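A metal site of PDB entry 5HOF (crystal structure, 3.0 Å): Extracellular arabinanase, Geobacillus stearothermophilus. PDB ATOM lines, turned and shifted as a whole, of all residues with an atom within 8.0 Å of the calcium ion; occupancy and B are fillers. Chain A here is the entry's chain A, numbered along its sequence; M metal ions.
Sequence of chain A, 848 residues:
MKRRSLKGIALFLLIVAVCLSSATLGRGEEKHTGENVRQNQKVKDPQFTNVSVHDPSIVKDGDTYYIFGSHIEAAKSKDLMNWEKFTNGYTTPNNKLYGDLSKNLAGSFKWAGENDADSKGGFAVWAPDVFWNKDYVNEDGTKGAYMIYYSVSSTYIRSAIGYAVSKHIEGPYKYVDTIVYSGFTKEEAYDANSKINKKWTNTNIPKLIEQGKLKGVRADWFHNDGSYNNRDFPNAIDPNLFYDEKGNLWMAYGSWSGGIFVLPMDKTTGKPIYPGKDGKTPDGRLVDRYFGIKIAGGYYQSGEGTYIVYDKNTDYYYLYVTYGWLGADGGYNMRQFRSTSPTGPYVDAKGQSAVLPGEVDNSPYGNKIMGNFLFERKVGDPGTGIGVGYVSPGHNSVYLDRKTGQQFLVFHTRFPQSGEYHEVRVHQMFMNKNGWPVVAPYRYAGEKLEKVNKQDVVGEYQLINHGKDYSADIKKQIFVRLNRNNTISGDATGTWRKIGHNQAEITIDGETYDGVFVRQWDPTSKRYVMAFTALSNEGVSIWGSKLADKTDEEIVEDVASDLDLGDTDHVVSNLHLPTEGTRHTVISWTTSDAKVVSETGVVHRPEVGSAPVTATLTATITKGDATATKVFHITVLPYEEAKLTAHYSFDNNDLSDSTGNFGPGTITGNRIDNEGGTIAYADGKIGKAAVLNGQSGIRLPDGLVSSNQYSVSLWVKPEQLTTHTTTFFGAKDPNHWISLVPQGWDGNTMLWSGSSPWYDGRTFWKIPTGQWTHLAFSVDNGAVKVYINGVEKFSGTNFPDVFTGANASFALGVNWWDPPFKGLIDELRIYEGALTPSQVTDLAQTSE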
ATOM      1  N   HIS A 647     -17.411 -20.161   6.629  1.00  0.00           N
ATOM      2  CA  HIS A 647     -18.072 -19.784   7.875  1.00  0.00           C
ATOM      3  C   HIS A 647     -17.867 -20.931   8.852  1.00  0.00           C
ATOM      4  O   HIS A 647     -18.517 -21.994   8.764  1.00  0.00           O
ATOM      5  CB  HIS A 647     -19.558 -19.484   7.624  1.00  0.00           C
ATOM      6  CG  HIS A 647     -20.361 -19.161   8.854  1.00  0.00           C
ATOM      7  ND1 HIS A 647     -21.743 -19.084   8.839  1.00  0.00           N
ATOM      8  CD2 HIS A 647     -19.995 -18.900  10.128  1.00  0.00           C
ATOM      9  CE1 HIS A 647     -22.184 -18.805  10.046  1.00  0.00           C
ATOM     10  NE2 HIS A 647     -21.144 -18.685  10.849  1.00  0.00           N
ATOM     11  N   TYR A 648     -16.920 -20.716   9.751  1.00  0.00           N
ATOM     12  CA  TYR A 648     -16.679 -21.588  10.881  1.00  0.00           C
ATOM     13  C   TYR A 648     -17.493 -20.991  12.039  1.00  0.00           C
ATOM     14  O   TYR A 648     -17.052 -20.075  12.743  1.00  0.00           O
ATOM     15  CB  TYR A 648     -15.175 -21.628  11.188  1.00  0.00           C
ATOM     16  CG  TYR A 648     -14.364 -22.208  10.028  1.00  0.00           C
ATOM     17  CD1 TYR A 648     -13.953 -21.421   8.952  1.00  0.00           C
ATOM     18  CD2 TYR A 648     -14.028 -23.561  10.010  1.00  0.00           C
ATOM     19  CE1 TYR A 648     -13.229 -21.970   7.890  1.00  0.00           C
ATOM     20  CE2 TYR A 648     -13.302 -24.118   8.970  1.00  0.00           C
ATOM     21  CZ  TYR A 648     -12.889 -23.329   7.909  1.00  0.00           C
ATOM     22  OH  TYR A 648     -12.149 -23.913   6.871  1.00  0.00           O
ATOM     23  N   SER A 649     -18.704 -21.501  12.182  1.00  0.00           N
ATOM     24  CA  SER A 649     -19.629 -21.003  13.195  1.00  0.00           C
ATOM     25  C   SER A 649     -19.409 -21.680  14.545  1.00  0.00           C
ATOM     26  O   SER A 649     -19.792 -21.137  15.597  1.00  0.00           O
ATOM     27  CB  SER A 649     -21.070 -21.218  12.743  1.00  0.00           C
ATOM     28  OG  SER A 649     -21.495 -22.534  12.982  1.00  0.00           O
ATOM     29  N   PHE A 650     -18.766 -22.862  14.517  1.00  0.00           N
ATOM     30  CA  PHE A 650     -18.582 -23.702  15.703  1.00  0.00           C
ATOM     31  C   PHE A 650     -19.920 -24.170  16.285  1.00  0.00           C
ATOM     32  O   PHE A 650     -20.012 -24.544  17.461  1.00  0.00           O
ATOM     33  CB  PHE A 650     -17.809 -22.952  16.787  1.00  0.00           C
ATOM     34  CG  PHE A 650     -16.592 -22.206  16.300  1.00  0.00           C
ATOM     35  CD1 PHE A 650     -15.506 -22.894  15.783  1.00  0.00           C
ATOM     36  CD2 PHE A 650     -16.522 -20.816  16.405  1.00  0.00           C
ATOM     37  CE1 PHE A 650     -14.379 -22.211  15.358  1.00  0.00           C
ATOM     38  CE2 PHE A 650     -15.389 -20.137  15.986  1.00  0.00           C
ATOM     39  CZ  PHE A 650     -14.326 -20.828  15.475  1.00  0.00           C
ATOM     40  N   ASP A 651     -20.970 -24.139  15.474  1.00  0.00           N
ATOM     41  CA  ASP A 651     -22.299 -24.294  15.989  1.00  0.00           C
ATOM     42  C   ASP A 651     -22.656 -25.752  16.216  1.00  0.00           C
ATOM     43  O   ASP A 651     -23.639 -26.043  16.894  1.00  0.00           O
ATOM     44  CB  ASP A 651     -23.328 -23.594  15.096  1.00  0.00           C
ATOM     45  CG  ASP A 651     -23.328 -22.075  15.295  1.00  0.00           C
ATOM     46  OD1 ASP A 651     -22.604 -21.622  16.210  1.00  0.00           O
ATOM     47  OD2 ASP A 651     -24.063 -21.362  14.564  1.00  0.00           O
ATOM     48  N   ASN A 652     -21.859 -26.673  15.659  1.00  0.00           N
ATOM     49  CA  ASN A 652     -22.090 -28.115  15.912  1.00  0.00           C
ATOM     50  C   ASN A 652     -20.931 -28.740  16.682  1.00  0.00           C
ATOM     51  O   ASN A 652     -20.571 -29.871  16.413  1.00  0.00           O
ATOM     52  CB  ASN A 652     -22.289 -28.881  14.609  1.00  0.00           C
ATOM     53  CG  ASN A 652     -23.149 -28.118  13.624  1.00  0.00           C
ATOM     54  OD1 ASN A 652     -24.116 -27.467  13.994  1.00  0.00           O
ATOM     55  ND2 ASN A 652     -22.765 -28.180  12.342  1.00  0.00           N
ATOM     56  N   TYR A 681     -16.357 -26.060  23.661  1.00  0.00           N
ATOM     57  CA  TYR A 681     -17.409 -25.308  22.982  1.00  0.00           C
ATOM     58  C   TYR A 681     -18.408 -24.806  24.008  1.00  0.00           C
ATOM     59  O   TYR A 681     -19.268 -25.541  24.451  1.00  0.00           O
ATOM     60  CB  TYR A 681     -18.112 -26.160  21.923  1.00  0.00           C
ATOM     61  CG  TYR A 681     -17.229 -26.555  20.756  1.00  0.00           C
ATOM     62  CD1 TYR A 681     -16.318 -27.608  20.862  1.00  0.00           C
ATOM     63  CD2 TYR A 681     -17.297 -25.878  19.546  1.00  0.00           C
ATOM     64  CE1 TYR A 681     -15.504 -27.974  19.790  1.00  0.00           C
ATOM     65  CE2 TYR A 681     -16.493 -26.235  18.474  1.00  0.00           C
ATOM     66  CZ  TYR A 681     -15.590 -27.287  18.603  1.00  0.00           C
ATOM     67  OH  TYR A 681     -14.788 -27.635  17.552  1.00  0.00           O
ATOM     68  N   ALA A 682     -18.241 -23.545  24.392  1.00  0.00           N
ATOM     69  CA  ALA A 682     -19.146 -22.834  25.287  1.00  0.00           C
ATOM     70  C   ALA A 682     -20.254 -22.126  24.487  1.00  0.00           C
ATOM     71  O   ALA A 682     -20.244 -22.106  23.259  1.00  0.00           O
ATOM     72  CB  ALA A 682     -18.374 -21.836  26.128  1.00  0.00           C
ATOM     73  N   ASP A 683     -21.222 -21.555  25.212  1.00  0.00           N
ATOM     74  CA  ASP A 683     -22.302 -20.782  24.600  1.00  0.00           C
ATOM     75  C   ASP A 683     -21.775 -19.456  24.050  1.00  0.00           C
ATOM     76  O   ASP A 683     -21.025 -18.738  24.721  1.00  0.00           O
ATOM     77  CB  ASP A 683     -23.448 -20.520  25.596  1.00  0.00           C
ATOM     78  CG  ASP A 683     -24.610 -19.760  24.965  1.00  0.00           C
ATOM     79  OD1 ASP A 683     -24.974 -20.082  23.817  1.00  0.00           O
ATOM     80  OD2 ASP A 683     -25.159 -18.841  25.630  1.00  0.00           O
ATOM     81  N   GLY A 684     -22.209 -19.130  22.832  1.00  0.00           N
ATOM     82  CA  GLY A 684     -21.625 -18.033  22.068  1.00  0.00           C
ATOM     83  C   GLY A 684     -22.535 -16.844  21.773  1.00  0.00           C
ATOM     84  O   GLY A 684     -23.678 -16.767  22.231  1.00  0.00           O
ATOM     85  N   LYS A 685     -21.989 -15.916  20.992  1.00  0.00           N
ATOM     86  CA  LYS A 685     -22.716 -14.728  20.584  1.00  0.00           C
ATOM     87  C   LYS A 685     -23.840 -15.154  19.657  1.00  0.00           C
ATOM     88  O   LYS A 685     -24.908 -14.576  19.649  1.00  0.00           O
ATOM     89  CB  LYS A 685     -21.778 -13.737  19.889  1.00  0.00           C
ATOM     90  CG  LYS A 685     -22.433 -12.513  19.330  1.00  0.00           C
ATOM     91  CD  LYS A 685     -23.122 -11.666  20.397  1.00  0.00           C
ATOM     92  CE  LYS A 685     -24.199 -10.799  19.733  1.00  0.00           C
ATOM     93  NZ  LYS A 685     -24.344  -9.394  20.238  1.00  0.00           N
ATOM     94  N   ILE A 686     -23.556 -16.167  18.844  1.00  0.00           N
ATOM     95  CA  ILE A 686     -24.549 -16.732  17.967  1.00  0.00           C
ATOM     96  C   ILE A 686     -24.356 -18.242  18.008  1.00  0.00           C
ATOM     97  O   ILE A 686     -23.411 -18.769  17.389  1.00  0.00           O
ATOM     98  CB  ILE A 686     -24.359 -16.212  16.531  1.00  0.00           C
ATOM     99  CG1 ILE A 686     -24.709 -14.720  16.492  1.00  0.00           C
ATOM    100  CG2 ILE A 686     -25.207 -17.030  15.536  1.00  0.00           C
ATOM    101  CD1 ILE A 686     -24.466 -14.057  15.162  1.00  0.00           C
ATOM    102  N   GLY A 687     -25.247 -18.925  18.731  1.00  0.00           N
ATOM    103  CA  GLY A 687     -25.074 -20.359  18.982  1.00  0.00           C
ATOM    104  C   GLY A 687     -23.813 -20.619  19.806  1.00  0.00           C
ATOM    105  O   GLY A 687     -23.398 -19.802  20.610  1.00  0.00           O
ATOM    106  N   LYS A 688     -23.166 -21.752  19.594  1.00  0.00           N
ATOM    107  CA  LYS A 688     -22.004 -22.052  20.398  1.00  0.00           C
ATOM    108  C   LYS A 688     -20.762 -21.369  19.836  1.00  0.00           C
ATOM    109  O   LYS A 688     -20.703 -21.038  18.651  1.00  0.00           O
ATOM    110  CB  LYS A 688     -21.808 -23.571  20.549  1.00  0.00           C
ATOM    111  CG  LYS A 688     -23.037 -24.242  21.180  1.00  0.00           C
ATOM    112  CD  LYS A 688     -22.684 -25.399  22.089  1.00  0.00           C
ATOM    113  CE  LYS A 688     -23.770 -25.671  23.124  1.00  0.00           C
ATOM    114  NZ  LYS A 688     -23.856 -24.624  24.186  1.00  0.00           N
ATOM    115  N   ALA A 689     -19.801 -21.129  20.721  1.00  0.00           N
ATOM    116  CA  ALA A 689     -18.540 -20.464  20.413  1.00  0.00           C
ATOM    117  C   ALA A 689     -17.384 -21.423  20.655  1.00  0.00           C
ATOM    118  O   ALA A 689     -17.508 -22.395  21.417  1.00  0.00           O
ATOM    119  CB  ALA A 689     -18.386 -19.239  21.293  1.00  0.00           C
ATOM    120  N   ALA A 690     -16.255 -21.165  20.000  1.00  0.00           N
ATOM    121  CA  ALA A 690     -15.016 -21.851  20.350  1.00  0.00           C
ATOM    122  C   ALA A 690     -14.508 -21.346  21.690  1.00  0.00           C
ATOM    123  O   ALA A 690     -14.896 -20.278  22.156  1.00  0.00           O
ATOM    124  CB  ALA A 690     -13.959 -21.617  19.290  1.00  0.00           C
ATOM    125  N   TRP A 715     -16.280 -12.426  15.996  1.00  0.00           N
ATOM    126  CA  TRP A 715     -16.793 -11.939  17.270  1.00  0.00           C
ATOM    127  C   TRP A 715     -15.908 -12.439  18.383  1.00  0.00           C
ATOM    128  O   TRP A 715     -15.783 -13.647  18.570  1.00  0.00           O
ATOM    129  CB  TRP A 715     -18.185 -12.505  17.492  1.00  0.00           C
ATOM    130  CG  TRP A 715     -19.314 -11.750  16.855  1.00  0.00           C
ATOM    131  CD1 TRP A 715     -19.919 -12.024  15.664  1.00  0.00           C
ATOM    132  CD2 TRP A 715     -20.005 -10.641  17.421  1.00  0.00           C
ATOM    133  NE1 TRP A 715     -20.942 -11.133  15.437  1.00  0.00           N
ATOM    134  CE2 TRP A 715     -21.017 -10.267  16.505  1.00  0.00           C
ATOM    135  CE3 TRP A 715     -19.872  -9.909  18.603  1.00  0.00           C
ATOM    136  CZ2 TRP A 715     -21.896  -9.199  16.747  1.00  0.00           C
ATOM    137  CZ3 TRP A 715     -20.740  -8.841  18.837  1.00  0.00           C
ATOM    138  CH2 TRP A 715     -21.725  -8.498  17.906  1.00  0.00           C
ATOM    139  N   TRP A 772     -18.643  -9.123  24.453  1.00  0.00           N
ATOM    140  CA  TRP A 772     -18.513  -9.431  23.031  1.00  0.00           C
ATOM    141  C   TRP A 772     -18.199  -8.134  22.291  1.00  0.00           C
ATOM    142  O   TRP A 772     -18.683  -7.052  22.649  1.00  0.00           O
ATOM    143  CB  TRP A 772     -19.787 -10.067  22.449  1.00  0.00           C
ATOM    144  CG  TRP A 772     -19.963 -11.517  22.838  1.00  0.00           C
ATOM    145  CD1 TRP A 772     -20.908 -12.025  23.668  1.00  0.00           C
ATOM    146  CD2 TRP A 772     -19.179 -12.646  22.397  1.00  0.00           C
ATOM    147  NE1 TRP A 772     -20.770 -13.390  23.768  1.00  0.00           N
ATOM    148  CE2 TRP A 772     -19.720 -13.796  23.002  1.00  0.00           C
ATOM    149  CE3 TRP A 772     -18.095 -12.803  21.534  1.00  0.00           C
ATOM    150  CZ2 TRP A 772     -19.197 -15.065  22.798  1.00  0.00           C
ATOM    151  CZ3 TRP A 772     -17.574 -14.085  21.325  1.00  0.00           C
ATOM    152  CH2 TRP A 772     -18.121 -15.191  21.960  1.00  0.00           C
ATOM    153  N   ILE A 825     -13.912 -17.150  20.562  1.00  0.00           N
ATOM    154  CA  ILE A 825     -14.003 -16.564  19.233  1.00  0.00           C
ATOM    155  C   ILE A 825     -15.261 -17.141  18.536  1.00  0.00           C
ATOM    156  O   ILE A 825     -15.476 -18.371  18.570  1.00  0.00           O
ATOM    157  CB  ILE A 825     -12.752 -16.917  18.443  1.00  0.00           C
ATOM    158  CG1 ILE A 825     -11.549 -16.161  19.040  1.00  0.00           C
ATOM    159  CG2 ILE A 825     -12.942 -16.630  16.961  1.00  0.00           C
ATOM    160  CD1 ILE A 825     -10.194 -16.503  18.412  1.00  0.00           C
ATOM    161  N   ASP A 826     -16.090 -16.285  17.916  1.00  0.00           N
ATOM    162  CA  ASP A 826     -17.332 -16.767  17.289  1.00  0.00           C
ATOM    163  C   ASP A 826     -17.569 -16.307  15.846  1.00  0.00           C
ATOM    164  O   ASP A 826     -17.057 -15.302  15.409  1.00  0.00           O
ATOM    165  CB  ASP A 826     -18.514 -16.387  18.149  1.00  0.00           C
ATOM    166  CG  ASP A 826     -19.729 -17.233  17.881  1.00  0.00           C
ATOM    167  OD1 ASP A 826     -19.588 -18.446  17.636  1.00  0.00           O
ATOM    168  OD2 ASP A 826     -20.844 -16.693  17.881  1.00  0.00           O
ATOM    169  N   GLU A 827     -18.352 -17.087  15.110  1.00  0.00           N
ATOM    170  CA  GLU A 827     -18.814 -16.737  13.755  1.00  0.00           C
ATOM    171  C   GLU A 827     -17.735 -16.163  12.913  1.00  0.00           C
ATOM    172  O   GLU A 827     -17.824 -14.992  12.507  1.00  0.00           O
ATOM    173  CB  GLU A 827     -19.990 -15.765  13.791  1.00  0.00           C
ATOM    174  CG  GLU A 827     -21.193 -16.252  14.577  1.00  0.00           C
ATOM    175  CD  GLU A 827     -21.692 -17.669  14.220  1.00  0.00           C
ATOM    176  OE1 GLU A 827     -22.291 -17.869  13.138  1.00  0.00           O
ATOM    177  OE2 GLU A 827     -21.535 -18.590  15.089  1.00  0.00           O
ATOM    178  N   LEU A 828     -16.713 -16.963  12.644  1.00  0.00           N
ATOM    179  CA  LEU A 828     -15.628 -16.504  11.776  1.00  0.00           C
ATOM    180  C   LEU A 828     -16.059 -16.574  10.330  1.00  0.00           C
ATOM    181  O   LEU A 828     -15.994 -17.644   9.734  1.00  0.00           O
ATOM    182  CB  LEU A 828     -14.388 -17.354  11.942  1.00  0.00           C
ATOM    183  CG  LEU A 828     -13.371 -17.070  10.830  1.00  0.00           C
ATOM    184  CD1 LEU A 828     -12.838 -15.653  10.991  1.00  0.00           C
ATOM    185  CD2 LEU A 828     -12.244 -18.111  10.828  1.00  0.00           C
HETATM  186 CA    CA M   1     -21.359 -19.743  16.772  1.00  0.00          CA
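Merely in contact with the calcium ion: Gly 687 (3.999 Å). Within 4 Å of the calcium ion: Ser 649, Asp 651, Ile 686, Gly 687, Lys 688, Asp 826 and Glu 827. The nearest printed residue that does not touch the calcium ion is Ala 689 (4.5 Å).
OE1 of Glu 827 sits at hydrogen-bond distance from NE2 of His 647, 2.7 Å away. N of Lys 685 is in hydrogen-bond range of OD2 of Asp 826, at 3.4 Å. The backbone carbonyl oxygen (O) of Trp 715 is in hydrogen-bond range of the backbone NH (N) of Asp 826 (2.7 Å).
The calcium ion is bound by OE2 of Glu 827 (2.0 Å), OD1 of Asp 651 (2.3 Å), O of Ile 686 (2.4 Å), OD1 of Asp 826 (2.4 Å), O of Lys 688 (2.4 Å) and O of Ser 649 (2.4 Å).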
